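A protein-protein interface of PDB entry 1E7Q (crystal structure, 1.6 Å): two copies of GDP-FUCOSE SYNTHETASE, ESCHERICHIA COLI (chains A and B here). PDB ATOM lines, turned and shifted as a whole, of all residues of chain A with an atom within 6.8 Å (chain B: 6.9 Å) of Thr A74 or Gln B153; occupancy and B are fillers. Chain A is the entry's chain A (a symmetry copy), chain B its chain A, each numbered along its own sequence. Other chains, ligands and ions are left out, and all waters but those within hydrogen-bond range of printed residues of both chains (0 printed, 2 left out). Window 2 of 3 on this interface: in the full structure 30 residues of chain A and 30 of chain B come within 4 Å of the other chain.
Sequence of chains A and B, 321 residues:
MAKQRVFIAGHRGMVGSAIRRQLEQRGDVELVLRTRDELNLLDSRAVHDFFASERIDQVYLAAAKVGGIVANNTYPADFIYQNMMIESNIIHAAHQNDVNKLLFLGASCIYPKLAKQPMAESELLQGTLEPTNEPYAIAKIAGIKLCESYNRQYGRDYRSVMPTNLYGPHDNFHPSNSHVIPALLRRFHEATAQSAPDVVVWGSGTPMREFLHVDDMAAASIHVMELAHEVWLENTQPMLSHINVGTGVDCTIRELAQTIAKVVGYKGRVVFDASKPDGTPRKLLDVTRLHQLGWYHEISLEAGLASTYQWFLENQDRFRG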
ATOM      1  N   GLY A  68      18.914  21.155  -1.887  1.00  0.00           N
ATOM      2  CA  GLY A  68      18.536  22.515  -1.662  1.00  0.00           C
ATOM      3  C   GLY A  68      18.032  23.209  -2.910  1.00  0.00           C
ATOM      4  O   GLY A  68      17.574  22.570  -3.884  1.00  0.00           O
ATOM      5  N   ILE A  69      18.009  24.547  -2.909  1.00  0.00           N
ATOM      6  CA  ILE A  69      17.355  25.315  -3.924  1.00  0.00           C
ATOM      7  C   ILE A  69      18.000  25.130  -5.306  1.00  0.00           C
ATOM      8  O   ILE A  69      17.345  24.976  -6.333  1.00  0.00           O
ATOM      9  CB  ILE A  69      17.066  26.750  -3.569  1.00  0.00           C
ATOM     10  CG1 ILE A  69      18.244  27.653  -3.375  1.00  0.00           C
ATOM     11  CG2 ILE A  69      16.134  26.923  -2.371  1.00  0.00           C
ATOM     12  CD1 ILE A  69      17.846  29.022  -2.812  1.00  0.00           C
ATOM     13  N   VAL A  70      19.344  25.229  -5.309  1.00  0.00           N
ATOM     14  CA  VAL A  70      20.046  25.073  -6.565  1.00  0.00           C
ATOM     15  C   VAL A  70      19.834  23.669  -7.114  1.00  0.00           C
ATOM     16  O   VAL A  70      19.499  23.500  -8.303  1.00  0.00           O
ATOM     17  CB  VAL A  70      21.541  25.386  -6.394  1.00  0.00           C
ATOM     18  CG1 VAL A  70      22.295  24.982  -7.659  1.00  0.00           C
ATOM     19  CG2 VAL A  70      21.792  26.823  -6.029  1.00  0.00           C
ATOM     20  N   ALA A  71      19.931  22.662  -6.236  1.00  0.00           N
ATOM     21  CA  ALA A  71      19.837  21.272  -6.730  1.00  0.00           C
ATOM     22  C   ALA A  71      18.459  21.062  -7.342  1.00  0.00           C
ATOM     23  O   ALA A  71      18.343  20.389  -8.370  1.00  0.00           O
ATOM     24  CB  ALA A  71      20.153  20.293  -5.601  1.00  0.00           C
ATOM     25  N   ASN A  72      17.403  21.423  -6.578  1.00  0.00           N
ATOM     26  CA  ASN A  72      16.056  21.122  -7.045  1.00  0.00           C
ATOM     27  C   ASN A  72      15.774  21.825  -8.391  1.00  0.00           C
ATOM     28  O   ASN A  72      14.951  21.326  -9.170  1.00  0.00           O
ATOM     29  CB  ASN A  72      14.997  21.581  -6.021  1.00  0.00           C
ATOM     30  CG  ASN A  72      14.773  20.455  -4.996  1.00  0.00           C
ATOM     31  OD1 ASN A  72      13.884  19.635  -5.219  1.00  0.00           O
ATOM     32  ND2 ASN A  72      15.509  20.395  -3.917  1.00  0.00           N
ATOM     33  N   ASN A  73      16.346  23.022  -8.613  1.00  0.00           N
ATOM     34  CA  ASN A  73      16.091  23.703  -9.892  1.00  0.00           C
ATOM     35  C   ASN A  73      17.037  23.222 -10.987  1.00  0.00           C
ATOM     36  O   ASN A  73      16.633  23.320 -12.154  1.00  0.00           O
ATOM     37  CB  ASN A  73      16.319  25.224  -9.743  1.00  0.00           C
ATOM     38  CG  ASN A  73      15.124  25.915  -9.137  1.00  0.00           C
ATOM     39  OD1 ASN A  73      14.035  26.029  -9.711  1.00  0.00           O
ATOM     40  ND2 ASN A  73      15.327  26.525  -7.987  1.00  0.00           N
ATOM     41  N   THR A  74      18.155  22.610 -10.615  1.00  0.00           N
ATOM     42  CA  THR A  74      19.140  22.219 -11.634  1.00  0.00           C
ATOM     43  C   THR A  74      18.938  20.808 -12.133  1.00  0.00           C
ATOM     44  O   THR A  74      19.133  20.517 -13.322  1.00  0.00           O
ATOM     45  CB  THR A  74      20.534  22.393 -10.998  1.00  0.00           C
ATOM     46  OG1 THR A  74      20.702  23.802 -10.708  1.00  0.00           O
ATOM     47  CG2 THR A  74      21.613  21.911 -11.916  1.00  0.00           C
ATOM     48  N   TYR A  75      18.446  19.934 -11.259  1.00  0.00           N
ATOM     49  CA  TYR A  75      18.220  18.538 -11.614  1.00  0.00           C
ATOM     50  C   TYR A  75      16.758  18.108 -11.355  1.00  0.00           C
ATOM     51  O   TYR A  75      16.516  17.096 -10.672  1.00  0.00           O
ATOM     52  CB  TYR A  75      19.157  17.697 -10.708  1.00  0.00           C
ATOM     53  CG  TYR A  75      20.621  18.080 -10.761  1.00  0.00           C
ATOM     54  CD1 TYR A  75      21.360  17.757 -11.879  1.00  0.00           C
ATOM     55  CD2 TYR A  75      21.213  18.897  -9.815  1.00  0.00           C
ATOM     56  CE1 TYR A  75      22.689  18.110 -11.992  1.00  0.00           C
ATOM     57  CE2 TYR A  75      22.556  19.239  -9.895  1.00  0.00           C
ATOM     58  CZ  TYR A  75      23.267  18.889 -11.033  1.00  0.00           C
ATOM     59  OH  TYR A  75      24.597  19.245 -11.193  1.00  0.00           O
ATOM     60  N   PRO A  76      15.788  18.782 -11.906  1.00  0.00           N
ATOM     61  CA  PRO A  76      14.391  18.459 -11.604  1.00  0.00           C
ATOM     62  C   PRO A  76      13.986  17.041 -11.946  1.00  0.00           C
ATOM     63  O   PRO A  76      13.247  16.382 -11.210  1.00  0.00           O
ATOM     64  CB  PRO A  76      13.584  19.525 -12.337  1.00  0.00           C
ATOM     65  CG  PRO A  76      14.518  19.897 -13.484  1.00  0.00           C
ATOM     66  CD  PRO A  76      15.935  19.948 -12.807  1.00  0.00           C
ATOM     67  N   ALA A  77      14.502  16.488 -13.053  1.00  0.00           N
ATOM     68  CA  ALA A  77      14.129  15.135 -13.456  1.00  0.00           C
ATOM     69  C   ALA A  77      14.647  14.123 -12.464  1.00  0.00           C
ATOM     70  O   ALA A  77      13.992  13.164 -12.075  1.00  0.00           O
ATOM     71  CB  ALA A  77      14.682  14.832 -14.853  1.00  0.00           C
ATOM     72  N   ASP A  78      15.875  14.378 -11.942  1.00  0.00           N
ATOM     73  CA  ASP A  78      16.430  13.421 -10.966  1.00  0.00           C
ATOM     74  C   ASP A  78      15.547  13.441  -9.685  1.00  0.00           C
ATOM     75  O   ASP A  78      15.264  12.380  -9.131  1.00  0.00           O
ATOM     76  CB  ASP A  78      17.848  13.842 -10.608  1.00  0.00           C
ATOM     77  CG  ASP A  78      18.830  13.623 -11.775  1.00  0.00           C
ATOM     78  OD1 ASP A  78      18.430  13.308 -12.938  1.00  0.00           O
ATOM     79  OD2 ASP A  78      19.912  14.170 -11.538  1.00  0.00           O
ATOM     80  N   PHE A  79      15.089  14.626  -9.271  1.00  0.00           N
ATOM     81  CA  PHE A  79      14.302  14.677  -8.023  1.00  0.00           C
ATOM     82  C   PHE A  79      12.899  14.060  -8.146  1.00  0.00           C
ATOM     83  O   PHE A  79      12.437  13.382  -7.230  1.00  0.00           O
ATOM     84  CB  PHE A  79      14.166  16.138  -7.548  1.00  0.00           C
ATOM     85  CG  PHE A  79      15.372  16.572  -6.794  1.00  0.00           C
ATOM     86  CD1 PHE A  79      15.498  16.305  -5.445  1.00  0.00           C
ATOM     87  CD2 PHE A  79      16.434  17.160  -7.491  1.00  0.00           C
ATOM     88  CE1 PHE A  79      16.640  16.676  -4.737  1.00  0.00           C
ATOM     89  CE2 PHE A  79      17.580  17.511  -6.770  1.00  0.00           C
ATOM     90  CZ  PHE A  79      17.674  17.329  -5.406  1.00  0.00           C
ATOM     91  N   HIS B  95      14.617   8.638 -22.423  1.00  0.00           N
ATOM     92  CA  HIS B  95      15.715   9.557 -22.237  1.00  0.00           C
ATOM     93  C   HIS B  95      17.074   8.865 -22.292  1.00  0.00           C
ATOM     94  O   HIS B  95      18.015   9.352 -22.940  1.00  0.00           O
ATOM     95  CB  HIS B  95      15.525  10.330 -20.913  1.00  0.00           C
ATOM     96  CG  HIS B  95      16.781  11.087 -20.635  1.00  0.00           C
ATOM     97  ND1 HIS B  95      17.177  12.213 -21.369  1.00  0.00           N
ATOM     98  CD2 HIS B  95      17.732  10.786 -19.700  1.00  0.00           C
ATOM     99  CE1 HIS B  95      18.360  12.598 -20.874  1.00  0.00           C
ATOM    100  NE2 HIS B  95      18.710  11.741 -19.921  1.00  0.00           N
ATOM    101  N   GLU B 148       7.890  17.447 -18.021  1.00  0.00           N
ATOM    102  CA  GLU B 148       8.422  18.791 -17.883  1.00  0.00           C
ATOM    103  C   GLU B 148       9.820  18.819 -17.239  1.00  0.00           C
ATOM    104  O   GLU B 148      10.668  19.581 -17.678  1.00  0.00           O
ATOM    105  CB  GLU B 148       7.475  19.667 -17.013  1.00  0.00           C
ATOM    106  CG  GLU B 148       6.140  19.859 -17.734  1.00  0.00           C
ATOM    107  CD  GLU B 148       5.097  20.596 -16.923  1.00  0.00           C
ATOM    108  OE1 GLU B 148       5.247  20.806 -15.706  1.00  0.00           O
ATOM    109  OE2 GLU B 148       4.066  20.898 -17.603  1.00  0.00           O
ATOM    110  N   SER B 149      10.058  17.880 -16.326  1.00  0.00           N
ATOM    111  CA  SER B 149      11.354  17.882 -15.632  1.00  0.00           C
ATOM    112  C   SER B 149      12.449  17.393 -16.575  1.00  0.00           C
ATOM    113  O   SER B 149      13.567  17.892 -16.513  1.00  0.00           O
ATOM    114  CB  SER B 149      11.229  17.024 -14.389  1.00  0.00           C
ATOM    115  OG  SER B 149      10.273  17.614 -13.480  1.00  0.00           O
ATOM    116  N   TYR B 150      12.176  16.375 -17.382  1.00  0.00           N
ATOM    117  CA  TYR B 150      13.139  15.922 -18.375  1.00  0.00           C
ATOM    118  C   TYR B 150      13.320  17.041 -19.439  1.00  0.00           C
ATOM    119  O   TYR B 150      14.469  17.207 -19.895  1.00  0.00           O
ATOM    120  CB  TYR B 150      12.736  14.605 -19.079  1.00  0.00           C
ATOM    121  CG  TYR B 150      13.071  13.375 -18.244  1.00  0.00           C
ATOM    122  CD1 TYR B 150      12.358  13.004 -17.132  1.00  0.00           C
ATOM    123  CD2 TYR B 150      14.245  12.699 -18.474  1.00  0.00           C
ATOM    124  CE1 TYR B 150      12.706  11.909 -16.351  1.00  0.00           C
ATOM    125  CE2 TYR B 150      14.643  11.607 -17.749  1.00  0.00           C
ATOM    126  CZ  TYR B 150      13.853  11.220 -16.666  1.00  0.00           C
ATOM    127  OH  TYR B 150      14.237  10.156 -15.889  1.00  0.00           O
ATOM    128  N   ASN B 151      12.271  17.749 -19.799  1.00  0.00           N
ATOM    129  CA  ASN B 151      12.433  18.858 -20.723  1.00  0.00           C
ATOM    130  C   ASN B 151      13.445  19.881 -20.175  1.00  0.00           C
ATOM    131  O   ASN B 151      14.339  20.379 -20.892  1.00  0.00           O
ATOM    132  CB  ASN B 151      11.111  19.535 -21.070  1.00  0.00           C
ATOM    133  CG  ASN B 151      10.218  18.601 -21.868  1.00  0.00           C
ATOM    134  OD1 ASN B 151      10.614  17.597 -22.432  1.00  0.00           O
ATOM    135  ND2 ASN B 151       8.939  19.034 -21.845  1.00  0.00           N
ATOM    136  N   ARG B 152      13.208  20.273 -18.924  1.00  0.00           N
ATOM    137  CA  ARG B 152      13.980  21.372 -18.331  1.00  0.00           C
ATOM    138  C   ARG B 152      15.394  20.927 -18.013  1.00  0.00           C
ATOM    139  O   ARG B 152      16.306  21.748 -18.195  1.00  0.00           O
ATOM    140  CB  ARG B 152      13.261  21.760 -17.035  1.00  0.00           C
ATOM    141  CG  ARG B 152      11.943  22.430 -17.308  1.00  0.00           C
ATOM    142  CD  ARG B 152      11.120  22.694 -16.057  1.00  0.00           C
ATOM    143  NE  ARG B 152      11.762  23.636 -15.152  1.00  0.00           N
ATOM    144  CZ  ARG B 152      11.977  23.468 -13.881  1.00  0.00           C
ATOM    145  NH1 ARG B 152      11.639  22.378 -13.152  1.00  0.00           N
ATOM    146  NH2 ARG B 152      12.625  24.484 -13.269  1.00  0.00           N
ATOM    147  N   GLN B 153      15.578  19.730 -17.484  1.00  0.00           N
ATOM    148  CA  GLN B 153      16.919  19.288 -17.081  1.00  0.00           C
ATOM    149  C   GLN B 153      17.779  18.923 -18.310  1.00  0.00           C
ATOM    150  O   GLN B 153      19.001  19.201 -18.342  1.00  0.00           O
ATOM    151  CB  GLN B 153      16.911  18.125 -16.140  1.00  0.00           C
ATOM    152  CG  GLN B 153      18.300  17.686 -15.667  1.00  0.00           C
ATOM    153  CD  GLN B 153      18.214  16.647 -14.565  1.00  0.00           C
ATOM    154  OE1 GLN B 153      17.209  16.533 -13.823  1.00  0.00           O
ATOM    155  NE2 GLN B 153      19.352  15.995 -14.274  1.00  0.00           N
ATOM    156  N   TYR B 154      17.203  18.181 -19.222  1.00  0.00           N
ATOM    157  CA  TYR B 154      17.939  17.617 -20.335  1.00  0.00           C
ATOM    158  C   TYR B 154      17.662  18.144 -21.729  1.00  0.00           C
ATOM    159  O   TYR B 154      18.321  17.716 -22.694  1.00  0.00           O
ATOM    160  CB  TYR B 154      17.652  16.106 -20.326  1.00  0.00           C
ATOM    161  CG  TYR B 154      18.102  15.348 -19.116  1.00  0.00           C
ATOM    162  CD1 TYR B 154      19.458  15.287 -18.786  1.00  0.00           C
ATOM    163  CD2 TYR B 154      17.191  14.750 -18.245  1.00  0.00           C
ATOM    164  CE1 TYR B 154      19.934  14.522 -17.754  1.00  0.00           C
ATOM    165  CE2 TYR B 154      17.662  13.994 -17.173  1.00  0.00           C
ATOM    166  CZ  TYR B 154      19.030  13.948 -16.916  1.00  0.00           C
ATOM    167  OH  TYR B 154      19.491  13.180 -15.858  1.00  0.00           O
ATOM    168  N   GLY B 155      16.771  19.124 -21.859  1.00  0.00           N
ATOM    169  CA  GLY B 155      16.430  19.706 -23.141  1.00  0.00           C
ATOM    170  C   GLY B 155      15.655  18.681 -23.989  1.00  0.00           C
ATOM    171  O   GLY B 155      15.673  18.896 -25.183  1.00  0.00           O
ATOM    172  N   ARG B 156      14.882  17.800 -23.389  1.00  0.00           N
ATOM    173  CA  ARG B 156      14.036  16.917 -24.181  1.00  0.00           C
ATOM    174  C   ARG B 156      12.807  17.703 -24.686  1.00  0.00           C
ATOM    175  O   ARG B 156      12.575  18.886 -24.440  1.00  0.00           O
ATOM    176  CB  ARG B 156      13.567  15.733 -23.321  1.00  0.00           C
ATOM    177  CG  ARG B 156      14.771  14.834 -22.978  1.00  0.00           C
ATOM    178  CD  ARG B 156      15.312  14.161 -24.228  1.00  0.00           C
ATOM    179  NE  ARG B 156      16.363  13.239 -23.853  1.00  0.00           N
ATOM    180  CZ  ARG B 156      17.298  12.928 -24.778  1.00  0.00           C
ATOM    181  NH1 ARG B 156      17.266  13.449 -26.015  1.00  0.00           N
ATOM    182  NH2 ARG B 156      18.279  12.091 -24.415  1.00  0.00           N
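The side-chain amide oxygen of Gln B153 lies close to the backbone carbonyl oxygen of Tyr A75 (3.3 Å).
N of Ala A77 sits at hydrogen-bond distance from OE1 of Gln B153 (2.8 Å).
The side-chain amide nitrogen (NE2) of Gln B153 sits at hydrogen-bond distance from the side-chain carboxylate (OD1) of Asp A78 (3.1 Å).
OH of Tyr B154 sits at hydrogen-bond distance from OD1 of Asp A78, at 3.1 Å.
N of Pro A76 sits close to OE1 of Gln B153 (3.3 Å).
NE2 of Gln B153 sits at hydrogen-bond distance from OH of Tyr B154 (3.2 Å).
The side-chain hydroxyl (OG1) of Thr A74 lies within hydrogen-bond range of the backbone carbonyl oxygen (O) of Val A70.
Thr A74 touches Gln B153 (O to CG, 3.8 Å).
Ser B149 touches Pro A76 (CB to C, 3.7 Å).
Pro A76 touches Arg B152 (CB to NH1, 3.5 Å).
Ser B149 touches Ala A77 (CB to N, 3.6 Å).
CB of Ala A77 touches CD1 of Tyr B150, at 3.7 Å.
CB of Ala A77 touches CE2 of Tyr B154, at 3.9 Å.
Thr A74 touches just one residue of chain B: Gln B153.
Printed residues of chain A within 4 Å of Ser B149: Pro A76 (3.7 Å) and Ala A77 (3.6 Å).
Of the printed residues of chain A, Arg B152 touches Pro A76 (3.5 Å).
Of chain A, only Thr A74 (3.8 Å), Tyr A75 (3.0 Å), Pro A76 (3.3 Å), Ala A77 (2.8 Å) and Asp A78 (3.1 Å) come within 4 Å of Gln B153.
Printed residues of chain A within 4 Å of Tyr B154: Ala A77 and Asp A78.
Gly B155 touches none of the printed residues of chain A.
The nearest residue of chain A that does not touch Gln B153 is Phe A79 (5.4 Å).
Printed residues of chain A that touch a printed residue of chain B: Thr A74, Tyr A75, Pro A76, Ala A77 and Asp A78.
Hydrophobic or aromatic side chains of chain A within 4 Å of the printed part of chain B: Tyr A75, Pro A76 and Ala A77.
Of the 10 printed residues of chain B, 5 touch a printed residue of chain A.
Hydrophobic or aromatic side chains of chain B that line the printed part of chain A: Tyr B150 and Tyr B154.
Among the printed residues, 11 pairs touch across the chains.
Among the printed residues, no Asp or Glu carboxylate lies within 4 Å of a Lys or Arg side-chain nitrogen of the other chain.
No position is printed for both chains.
Of the 11 pairs that touch across the chains among the printed residues, none has its exchanged pair printed and touching as well.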
